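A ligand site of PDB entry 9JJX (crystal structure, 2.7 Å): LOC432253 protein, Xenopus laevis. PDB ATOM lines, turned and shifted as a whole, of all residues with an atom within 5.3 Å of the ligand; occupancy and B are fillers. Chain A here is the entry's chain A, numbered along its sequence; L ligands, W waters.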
ATOM      1  N   GLU A  47     -15.004  -3.787   6.705  1.00  0.00           N
ATOM      2  CA  GLU A  47     -16.011  -4.736   6.190  1.00  0.00           C
ATOM      3  C   GLU A  47     -16.881  -4.001   5.172  1.00  0.00           C
ATOM      4  O   GLU A  47     -16.956  -2.772   5.266  1.00  0.00           O
ATOM      5  CB  GLU A  47     -16.859  -5.296   7.336  1.00  0.00           C
ATOM      6  CG  GLU A  47     -16.057  -6.102   8.337  1.00  0.00           C
ATOM      7  CD  GLU A  47     -16.877  -6.670   9.475  1.00  0.00           C
ATOM      8  OE1 GLU A  47     -18.117  -6.514   9.447  1.00  0.00           O
ATOM      9  OE2 GLU A  47     -16.288  -7.266  10.397  1.00  0.00           O
ATOM     10  N   LYS A  48     -17.482  -4.733   4.249  1.00  0.00           N
ATOM     11  CA  LYS A  48     -18.334  -4.186   3.214  1.00  0.00           C
ATOM     12  C   LYS A  48     -19.694  -3.796   3.798  1.00  0.00           C
ATOM     13  O   LYS A  48     -20.112  -4.300   4.843  1.00  0.00           O
ATOM     14  CB  LYS A  48     -18.514  -5.185   2.074  1.00  0.00           C
ATOM     15  CG  LYS A  48     -19.661  -4.855   1.130  1.00  0.00           C
ATOM     16  CD  LYS A  48     -19.532  -5.545  -0.218  1.00  0.00           C
ATOM     17  CE  LYS A  48     -19.851  -4.579  -1.351  1.00  0.00           C
ATOM     18  NZ  LYS A  48     -19.677  -5.204  -2.680  1.00  0.00           N
ATOM     19  N   ARG A  49     -20.364  -2.870   3.125  1.00  0.00           N
ATOM     20  CA  ARG A  49     -21.702  -2.433   3.516  1.00  0.00           C
ATOM     21  C   ARG A  49     -21.675  -1.741   4.878  1.00  0.00           C
ATOM     22  O   ARG A  49     -22.603  -1.880   5.675  1.00  0.00           O
ATOM     23  CB  ARG A  49     -22.682  -3.602   3.522  1.00  0.00           C
ATOM     24  CG  ARG A  49     -22.660  -4.451   2.260  1.00  0.00           C
ATOM     25  CD  ARG A  49     -23.216  -5.842   2.524  1.00  0.00           C
ATOM     26  NE  ARG A  49     -23.151  -6.704   1.347  1.00  0.00           N
ATOM     27  CZ  ARG A  49     -23.541  -7.968   1.322  1.00  0.00           C
ATOM     28  NH1 ARG A  49     -24.030  -8.563   2.399  1.00  0.00           N
ATOM     29  NH2 ARG A  49     -23.447  -8.658   0.186  1.00  0.00           N
ATOM     30  N   ARG A  50     -20.604  -0.985   5.138  1.00  0.00           N
ATOM     31  CA  ARG A  50     -20.480  -0.254   6.386  1.00  0.00           C
ATOM     32  C   ARG A  50     -20.231   1.237   6.194  1.00  0.00           C
ATOM     33  O   ARG A  50     -20.149   1.966   7.193  1.00  0.00           O
ATOM     34  CB  ARG A  50     -19.350  -0.856   7.241  1.00  0.00           C
ATOM     35  CG  ARG A  50     -19.759  -2.070   8.052  1.00  0.00           C
ATOM     36  CD  ARG A  50     -21.229  -1.988   8.449  1.00  0.00           C
ATOM     37  NE  ARG A  50     -21.597  -3.003   9.428  1.00  0.00           N
ATOM     38  CZ  ARG A  50     -21.495  -4.311   9.243  1.00  0.00           C
ATOM     39  NH1 ARG A  50     -21.034  -4.818   8.112  1.00  0.00           N
ATOM     40  NH2 ARG A  50     -21.864  -5.140  10.221  1.00  0.00           N
ATOM     41  N   GLY A  51     -20.102   1.712   4.965  1.00  0.00           N
ATOM     42  CA  GLY A  51     -19.976   3.120   4.688  1.00  0.00           C
ATOM     43  C   GLY A  51     -18.590   3.622   4.358  1.00  0.00           C
ATOM     44  O   GLY A  51     -18.329   4.821   4.524  1.00  0.00           O
ATOM     45  N   LYS A  52     -17.688   2.759   3.892  1.00  0.00           N
ATOM     46  CA  LYS A  52     -16.331   3.202   3.556  1.00  0.00           C
ATOM     47  C   LYS A  52     -16.341   4.143   2.359  1.00  0.00           C
ATOM     48  O   LYS A  52     -15.782   5.246   2.419  1.00  0.00           O
ATOM     49  CB  LYS A  52     -15.436   1.983   3.297  1.00  0.00           C
ATOM     50  CG  LYS A  52     -15.338   1.032   4.473  1.00  0.00           C
ATOM     51  CD  LYS A  52     -14.176   0.048   4.308  1.00  0.00           C
ATOM     52  CE  LYS A  52     -14.286  -0.729   3.005  1.00  0.00           C
ATOM     53  NZ  LYS A  52     -15.421  -1.690   3.018  1.00  0.00           N
ATOM     54  N   SER A  53     -16.971   3.718   1.259  1.00  0.00           N
ATOM     55  CA  SER A  53     -17.036   4.568   0.075  1.00  0.00           C
ATOM     56  C   SER A  53     -17.805   5.859   0.361  1.00  0.00           C
ATOM     57  O   SER A  53     -17.467   6.924  -0.181  1.00  0.00           O
ATOM     58  CB  SER A  53     -17.692   3.802  -1.075  1.00  0.00           C
ATOM     59  OG  SER A  53     -17.107   2.520  -1.223  1.00  0.00           O
ATOM     60  N   PHE A  54     -18.830   5.790   1.200  1.00  0.00           N
ATOM     61  CA  PHE A  54     -19.592   6.972   1.579  1.00  0.00           C
ATOM     62  C   PHE A  54     -18.696   8.013   2.252  1.00  0.00           C
ATOM     63  O   PHE A  54     -18.657   9.186   1.837  1.00  0.00           O
ATOM     64  CB  PHE A  54     -20.726   6.532   2.520  1.00  0.00           C
ATOM     65  CG  PHE A  54     -21.669   7.628   2.916  1.00  0.00           C
ATOM     66  CD1 PHE A  54     -21.443   8.391   4.040  1.00  0.00           C
ATOM     67  CD2 PHE A  54     -22.816   7.873   2.164  1.00  0.00           C
ATOM     68  CE1 PHE A  54     -22.314   9.391   4.407  1.00  0.00           C
ATOM     69  CE2 PHE A  54     -23.691   8.868   2.523  1.00  0.00           C
ATOM     70  CZ  PHE A  54     -23.443   9.631   3.649  1.00  0.00           C
ATOM     71  N   PHE A  84     -20.587   3.790  -3.687  1.00  0.00           N
ATOM     72  CA  PHE A  84     -21.983   3.371  -3.653  1.00  0.00           C
ATOM     73  C   PHE A  84     -22.930   4.525  -3.396  1.00  0.00           C
ATOM     74  O   PHE A  84     -23.943   4.657  -4.099  1.00  0.00           O
ATOM     75  CB  PHE A  84     -22.180   2.288  -2.580  1.00  0.00           C
ATOM     76  CG  PHE A  84     -23.436   1.476  -2.751  1.00  0.00           C
ATOM     77  CD1 PHE A  84     -24.653   2.086  -2.996  1.00  0.00           C
ATOM     78  CD2 PHE A  84     -23.386   0.102  -2.682  1.00  0.00           C
ATOM     79  CE1 PHE A  84     -25.790   1.337  -3.157  1.00  0.00           C
ATOM     80  CE2 PHE A  84     -24.527  -0.660  -2.847  1.00  0.00           C
ATOM     81  CZ  PHE A  84     -25.728  -0.044  -3.078  1.00  0.00           C
ATOM     82  N   LYS A  85     -22.625   5.371  -2.414  1.00  0.00           N
ATOM     83  CA  LYS A  85     -23.400   6.575  -2.138  1.00  0.00           C
ATOM     84  C   LYS A  85     -23.859   7.204  -3.455  1.00  0.00           C
ATOM     85  O   LYS A  85     -24.978   7.724  -3.537  1.00  0.00           O
ATOM     86  CB  LYS A  85     -22.553   7.542  -1.304  1.00  0.00           C
ATOM     87  CG  LYS A  85     -23.133   8.930  -1.094  1.00  0.00           C
ATOM     88  CD  LYS A  85     -22.078   9.849  -0.499  1.00  0.00           C
ATOM     89  CE  LYS A  85     -22.449  11.319  -0.647  1.00  0.00           C
ATOM     90  NZ  LYS A  85     -21.452  12.044  -1.484  1.00  0.00           N
ATOM     91  N   ASP A 119      -9.622   3.383  -1.825  1.00  0.00           N
ATOM     92  CA  ASP A 119     -10.679   2.583  -1.226  1.00  0.00           C
ATOM     93  C   ASP A 119     -10.337   1.117  -1.434  1.00  0.00           C
ATOM     94  O   ASP A 119     -10.008   0.702  -2.555  1.00  0.00           O
ATOM     95  CB  ASP A 119     -12.032   2.916  -1.847  1.00  0.00           C
ATOM     96  CG  ASP A 119     -13.195   2.443  -1.009  1.00  0.00           C
ATOM     97  OD1 ASP A 119     -13.005   1.525  -0.174  1.00  0.00           O
ATOM     98  OD2 ASP A 119     -14.316   2.978  -1.184  1.00  0.00           O
ATOM     99  N   GLU A 121     -12.130  -1.778  -1.526  1.00  0.00           N
ATOM    100  CA  GLU A 121     -13.358  -2.539  -1.725  1.00  0.00           C
ATOM    101  C   GLU A 121     -12.988  -4.007  -1.872  1.00  0.00           C
ATOM    102  O   GLU A 121     -12.555  -4.458  -2.935  1.00  0.00           O
ATOM    103  CB  GLU A 121     -14.111  -2.040  -2.962  1.00  0.00           C
ATOM    104  CG  GLU A 121     -15.593  -1.780  -2.741  1.00  0.00           C
ATOM    105  CD  GLU A 121     -15.857  -0.703  -1.712  1.00  0.00           C
ATOM    106  OE1 GLU A 121     -14.935   0.087  -1.403  1.00  0.00           O
ATOM    107  OE2 GLU A 121     -16.995  -0.637  -1.200  1.00  0.00           O
ATOM    108  N   ARG A 186     -18.585   2.460  13.466  1.00  0.00           N
ATOM    109  CA  ARG A 186     -19.841   2.866  12.847  1.00  0.00           C
ATOM    110  C   ARG A 186     -21.025   2.317  13.613  1.00  0.00           C
ATOM    111  O   ARG A 186     -20.977   1.207  14.151  1.00  0.00           O
ATOM    112  CB  ARG A 186     -19.906   2.402  11.392  1.00  0.00           C
ATOM    113  CG  ARG A 186     -18.670   2.737  10.571  1.00  0.00           C
ATOM    114  CD  ARG A 186     -18.554   4.234  10.324  1.00  0.00           C
ATOM    115  NE  ARG A 186     -19.504   4.708   9.324  1.00  0.00           N
ATOM    116  CZ  ARG A 186     -19.190   5.014   8.079  1.00  0.00           C
ATOM    117  NH1 ARG A 186     -17.949   4.903   7.630  1.00  0.00           N
ATOM    118  NH2 ARG A 186     -20.145   5.439   7.254  1.00  0.00           N
ATOM    119  N   ASP A 187     -22.106   3.098  13.666  1.00  0.00           N
ATOM    120  CA  ASP A 187     -23.370   2.683  14.286  1.00  0.00           C
ATOM    121  C   ASP A 187     -23.160   2.255  15.740  1.00  0.00           C
ATOM    122  O   ASP A 187     -23.779   1.298  16.215  1.00  0.00           O
ATOM    123  CB  ASP A 187     -24.033   1.565  13.488  1.00  0.00           C
ATOM    124  CG  ASP A 187     -24.001   1.833  11.987  1.00  0.00           C
ATOM    125  OD1 ASP A 187     -23.718   2.976  11.587  1.00  0.00           O
ATOM    126  OD2 ASP A 187     -24.272   0.894  11.209  1.00  0.00           O
ATOM    127  N   LEU A 233     -19.068   7.404  15.323  1.00  0.00           N
ATOM    128  CA  LEU A 233     -20.180   8.163  14.779  1.00  0.00           C
ATOM    129  C   LEU A 233     -21.475   7.364  14.899  1.00  0.00           C
ATOM    130  O   LEU A 233     -21.457   6.130  14.944  1.00  0.00           O
ATOM    131  CB  LEU A 233     -19.940   8.528  13.303  1.00  0.00           C
ATOM    132  CG  LEU A 233     -19.558   7.365  12.389  1.00  0.00           C
ATOM    133  CD1 LEU A 233     -19.998   7.646  10.959  1.00  0.00           C
ATOM    134  CD2 LEU A 233     -18.060   7.102  12.444  1.00  0.00           C
ATOM    135  N   PRO A 234     -22.623   8.052  14.960  1.00  0.00           N
ATOM    136  CA  PRO A 234     -23.890   7.337  15.168  1.00  0.00           C
ATOM    137  C   PRO A 234     -24.370   6.610  13.919  1.00  0.00           C
ATOM    138  O   PRO A 234     -23.637   6.478  12.940  1.00  0.00           O
ATOM    139  CB  PRO A 234     -24.858   8.466  15.558  1.00  0.00           C
ATOM    140  CG  PRO A 234     -24.318   9.655  14.847  1.00  0.00           C
ATOM    141  CD  PRO A 234     -22.817   9.505  14.876  1.00  0.00           C
ATOM    142  N   HIS A 235     -25.608   6.124  13.967  1.00  0.00           N
ATOM    143  CA  HIS A 235     -26.210   5.499  12.790  1.00  0.00           C
ATOM    144  C   HIS A 235     -26.528   6.557  11.754  1.00  0.00           C
ATOM    145  O   HIS A 235     -26.951   7.671  12.102  1.00  0.00           O
ATOM    146  CB  HIS A 235     -27.475   4.736  13.195  1.00  0.00           C
ATOM    147  CG  HIS A 235     -27.941   3.760  12.159  1.00  0.00           C
ATOM    148  ND1 HIS A 235     -28.834   4.089  11.162  1.00  0.00           N
ATOM    149  CD2 HIS A 235     -27.656   2.446  11.980  1.00  0.00           C
ATOM    150  CE1 HIS A 235     -29.068   3.031  10.407  1.00  0.00           C
ATOM    151  NE2 HIS A 235     -28.359   2.023  10.887  1.00  0.00           N
ATOM    152  N   PRO A 236     -26.345   6.266  10.461  1.00  0.00           N
ATOM    153  CA  PRO A 236     -26.590   7.293   9.445  1.00  0.00           C
ATOM    154  C   PRO A 236     -28.043   7.737   9.370  1.00  0.00           C
ATOM    155  O   PRO A 236     -28.321   8.809   8.822  1.00  0.00           O
ATOM    156  CB  PRO A 236     -26.155   6.607   8.142  1.00  0.00           C
ATOM    157  CG  PRO A 236     -26.316   5.139   8.429  1.00  0.00           C
ATOM    158  CD  PRO A 236     -25.922   4.987   9.872  1.00  0.00           C
ATOM    159  N   ILE A 240     -30.105   7.557   4.765  1.00  0.00           N
ATOM    160  CA  ILE A 240     -28.939   7.063   4.067  1.00  0.00           C
ATOM    161  C   ILE A 240     -29.030   5.563   3.816  1.00  0.00           C
ATOM    162  O   ILE A 240     -28.711   5.091   2.718  1.00  0.00           O
ATOM    163  CB  ILE A 240     -27.657   7.420   4.838  1.00  0.00           C
ATOM    164  CG1 ILE A 240     -27.345   8.909   4.715  1.00  0.00           C
ATOM    165  CG2 ILE A 240     -26.483   6.569   4.366  1.00  0.00           C
ATOM    166  CD1 ILE A 240     -27.595   9.465   3.333  1.00  0.00           C
ATOM    167  N   THR A 241     -29.468   4.805   4.823  1.00  0.00           N
ATOM    168  CA  THR A 241     -29.604   3.361   4.659  1.00  0.00           C
ATOM    169  C   THR A 241     -30.620   3.046   3.575  1.00  0.00           C
ATOM    170  O   THR A 241     -31.700   3.628   3.528  1.00  0.00           O
ATOM    171  CB  THR A 241     -30.012   2.716   5.983  1.00  0.00           C
ATOM    172  OG1 THR A 241     -29.410   3.430   7.075  1.00  0.00           O
ATOM    173  CG2 THR A 241     -29.569   1.269   6.024  1.00  0.00           C
ATOM    174  N   GLY A 242     -30.270   2.109   2.701  1.00  0.00           N
ATOM    175  CA  GLY A 242     -31.103   1.804   1.567  1.00  0.00           C
ATOM    176  C   GLY A 242     -31.081   2.917   0.531  1.00  0.00           C
ATOM    177  O   GLY A 242     -30.199   3.775   0.492  1.00  0.00           O
ATOM    178  N   PHE A 255     -25.400  12.454  13.060  1.00  0.00           N
ATOM    179  CA  PHE A 255     -24.482  11.849  12.105  1.00  0.00           C
ATOM    180  C   PHE A 255     -23.827  12.900  11.222  1.00  0.00           C
ATOM    181  O   PHE A 255     -22.627  12.819  10.934  1.00  0.00           O
ATOM    182  CB  PHE A 255     -25.215  10.818  11.243  1.00  0.00           C
ATOM    183  CG  PHE A 255     -24.367  10.215  10.160  1.00  0.00           C
ATOM    184  CD1 PHE A 255     -23.522   9.148  10.428  1.00  0.00           C
ATOM    185  CD2 PHE A 255     -24.410  10.721   8.870  1.00  0.00           C
ATOM    186  CE1 PHE A 255     -22.731   8.600   9.427  1.00  0.00           C
ATOM    187  CE2 PHE A 255     -23.619  10.173   7.869  1.00  0.00           C
ATOM    188  CZ  PHE A 255     -22.789   9.115   8.150  1.00  0.00           C
HETATM  189  P1  LIG L   1     -18.468   0.036   1.688  1.00  0.00           P
HETATM  190  O1  LIG L   1     -17.752  -0.600   2.784  1.00  0.00           O
HETATM  191  O2  LIG L   1     -18.868  -1.064   0.811  1.00  0.00           O
HETATM  192  O3  LIG L   1     -17.458   0.760   0.931  1.00  0.00           O
HETATM  193  O4  LIG L   1     -19.732   0.968   2.182  1.00  0.00           O
HETATM  194  P2  LIG L   1     -20.687   1.762   1.111  1.00  0.00           P
HETATM  195  O5  LIG L   1     -20.146   3.077   0.795  1.00  0.00           O
HETATM  196  O6  LIG L   1     -20.710   1.110  -0.201  1.00  0.00           O
HETATM  197  O7  LIG L   1     -22.202   1.903   1.739  1.00  0.00           O
HETATM  198  C1  LIG L   1     -22.990   0.770   1.921  1.00  0.00           C
HETATM  199  C2  LIG L   1     -24.316   1.287   2.312  1.00  0.00           C
HETATM  200  O8  LIG L   1     -24.320   1.583   3.767  1.00  0.00           O
HETATM  201  C3  LIG L   1     -24.537   2.560   1.581  1.00  0.00           C
HETATM  202  O9  LIG L   1     -25.768   2.512   0.829  1.00  0.00           O
HETATM  203  C4  LIG L   1     -24.584   3.646   2.568  1.00  0.00           C
HETATM  204  O10 LIG L   1     -25.698   4.524   2.304  1.00  0.00           O
HETATM  205  C5  LIG L   1     -24.763   3.003   3.898  1.00  0.00           C
HETATM  206  N1  LIG L   1     -24.042   3.697   4.898  1.00  0.00           N
HETATM  207  C6  LIG L   1     -23.358   4.724   4.576  1.00  0.00           C
HETATM  208  N2  LIG L   1     -22.772   5.207   5.726  1.00  0.00           N
HETATM  209  C7  LIG L   1     -23.246   4.262   6.825  1.00  0.00           C
HETATM  210  C8  LIG L   1     -23.096   4.061   8.295  1.00  0.00           C
HETATM  211  O11 LIG L   1     -22.301   4.936   9.042  1.00  0.00           O
HETATM  212  N3  LIG L   1     -23.739   3.025   8.909  1.00  0.00           N
HETATM  213  C9  LIG L   1     -24.542   2.141   8.145  1.00  0.00           C
HETATM  214  N4  LIG L   1     -25.205   1.042   8.826  1.00  0.00           N
HETATM  215  N5  LIG L   1     -24.720   2.260   6.806  1.00  0.00           N
HETATM  216  C10 LIG L   1     -24.092   3.301   6.098  1.00  0.00           C
HETATM  217  O   HOH W   1     -26.671  -0.144   4.249  1.00  0.00           O
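The backbone carbonyl oxygen (O) of Glu 47 lies close to an oxygen (O1) of the ligand (3.4 Å). Residues that only touch the ligand: Phe 84 (3.0 Å), Pro 236 (3.1 Å), Arg 50 (3.6 Å), Lys 48 (3.7 Å), Phe 255 (3.7 Å) and His 235 (3.9 Å). Hydrophobic or aromatic side chains that line the ligand: Phe 54, Phe 84, Pro 236, Ile 240 and Phe 255.
The side-chain carboxylate of Glu 47 is in salt-bridge range of the guanidinium group of Arg 50. The backbone carbonyl oxygen of Glu 47 sits at hydrogen-bond distance from the side-chain amino group of Lys 52 (2.9 Å). The backbone NH (N) of Asp 187 sits at hydrogen-bond distance from the backbone carbonyl oxygen (O) of Leu 233. The backbone carbonyl oxygen (O) of Gly 51 sits at hydrogen-bond distance from the guanidinium group (NH1) of Arg 186, 3.1 Å away. The side-chain carboxylate (OE2) of Glu 121 lies within hydrogen-bond range of the side-chain hydroxyl (OG) of Ser 53 (3.2 Å). OG of Ser 53 lies within hydrogen-bond range of OD2 of Asp 119, at 2.8 Å. The side-chain carboxylate (OE1) of Glu 121 lies close to the side-chain carboxylate (OD1) of Asp 119. The backbone carbonyl oxygen (O) of Arg 50 sits close to the guanidinium group (NH2) of Arg 186, 3.5 Å away.
An oxygen (O3) of the ligand is in hydrogen-bond range of the side-chain hydroxyl (OG) of Ser 53. A nitrogen (N4) of the ligand is in hydrogen-bond range of the side-chain carboxylate of Asp 187 (2.6 Å). O4 of the ligand sits at hydrogen-bond distance from N of Gly 51 (2.9 Å). N of Phe 54 sits at hydrogen-bond distance from O5 of the ligand (3.0 Å). O of Ile 240 sits close to O10 of the ligand (3.1 Å). NE of Arg 186 lies within hydrogen-bond range of O11 of the ligand, 2.8 Å away. O3 of the ligand sits close to OE2 of Glu 121, at 2.6 Å. NZ of Lys 52 is in salt-bridge range of O1 of the ligand (2.6 Å). The backbone NH (N) of Ser 53 is in hydrogen-bond range of an oxygen (O3) of the ligand, at 3.0 Å. An oxygen (O4) of the ligand is in hydrogen-bond range of the backbone NH of Lys 52 (3.2 Å). An oxygen (O2) of the ligand is in hydrogen-bond range of the backbone NH (N) of Arg 49, at 3.3 Å.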
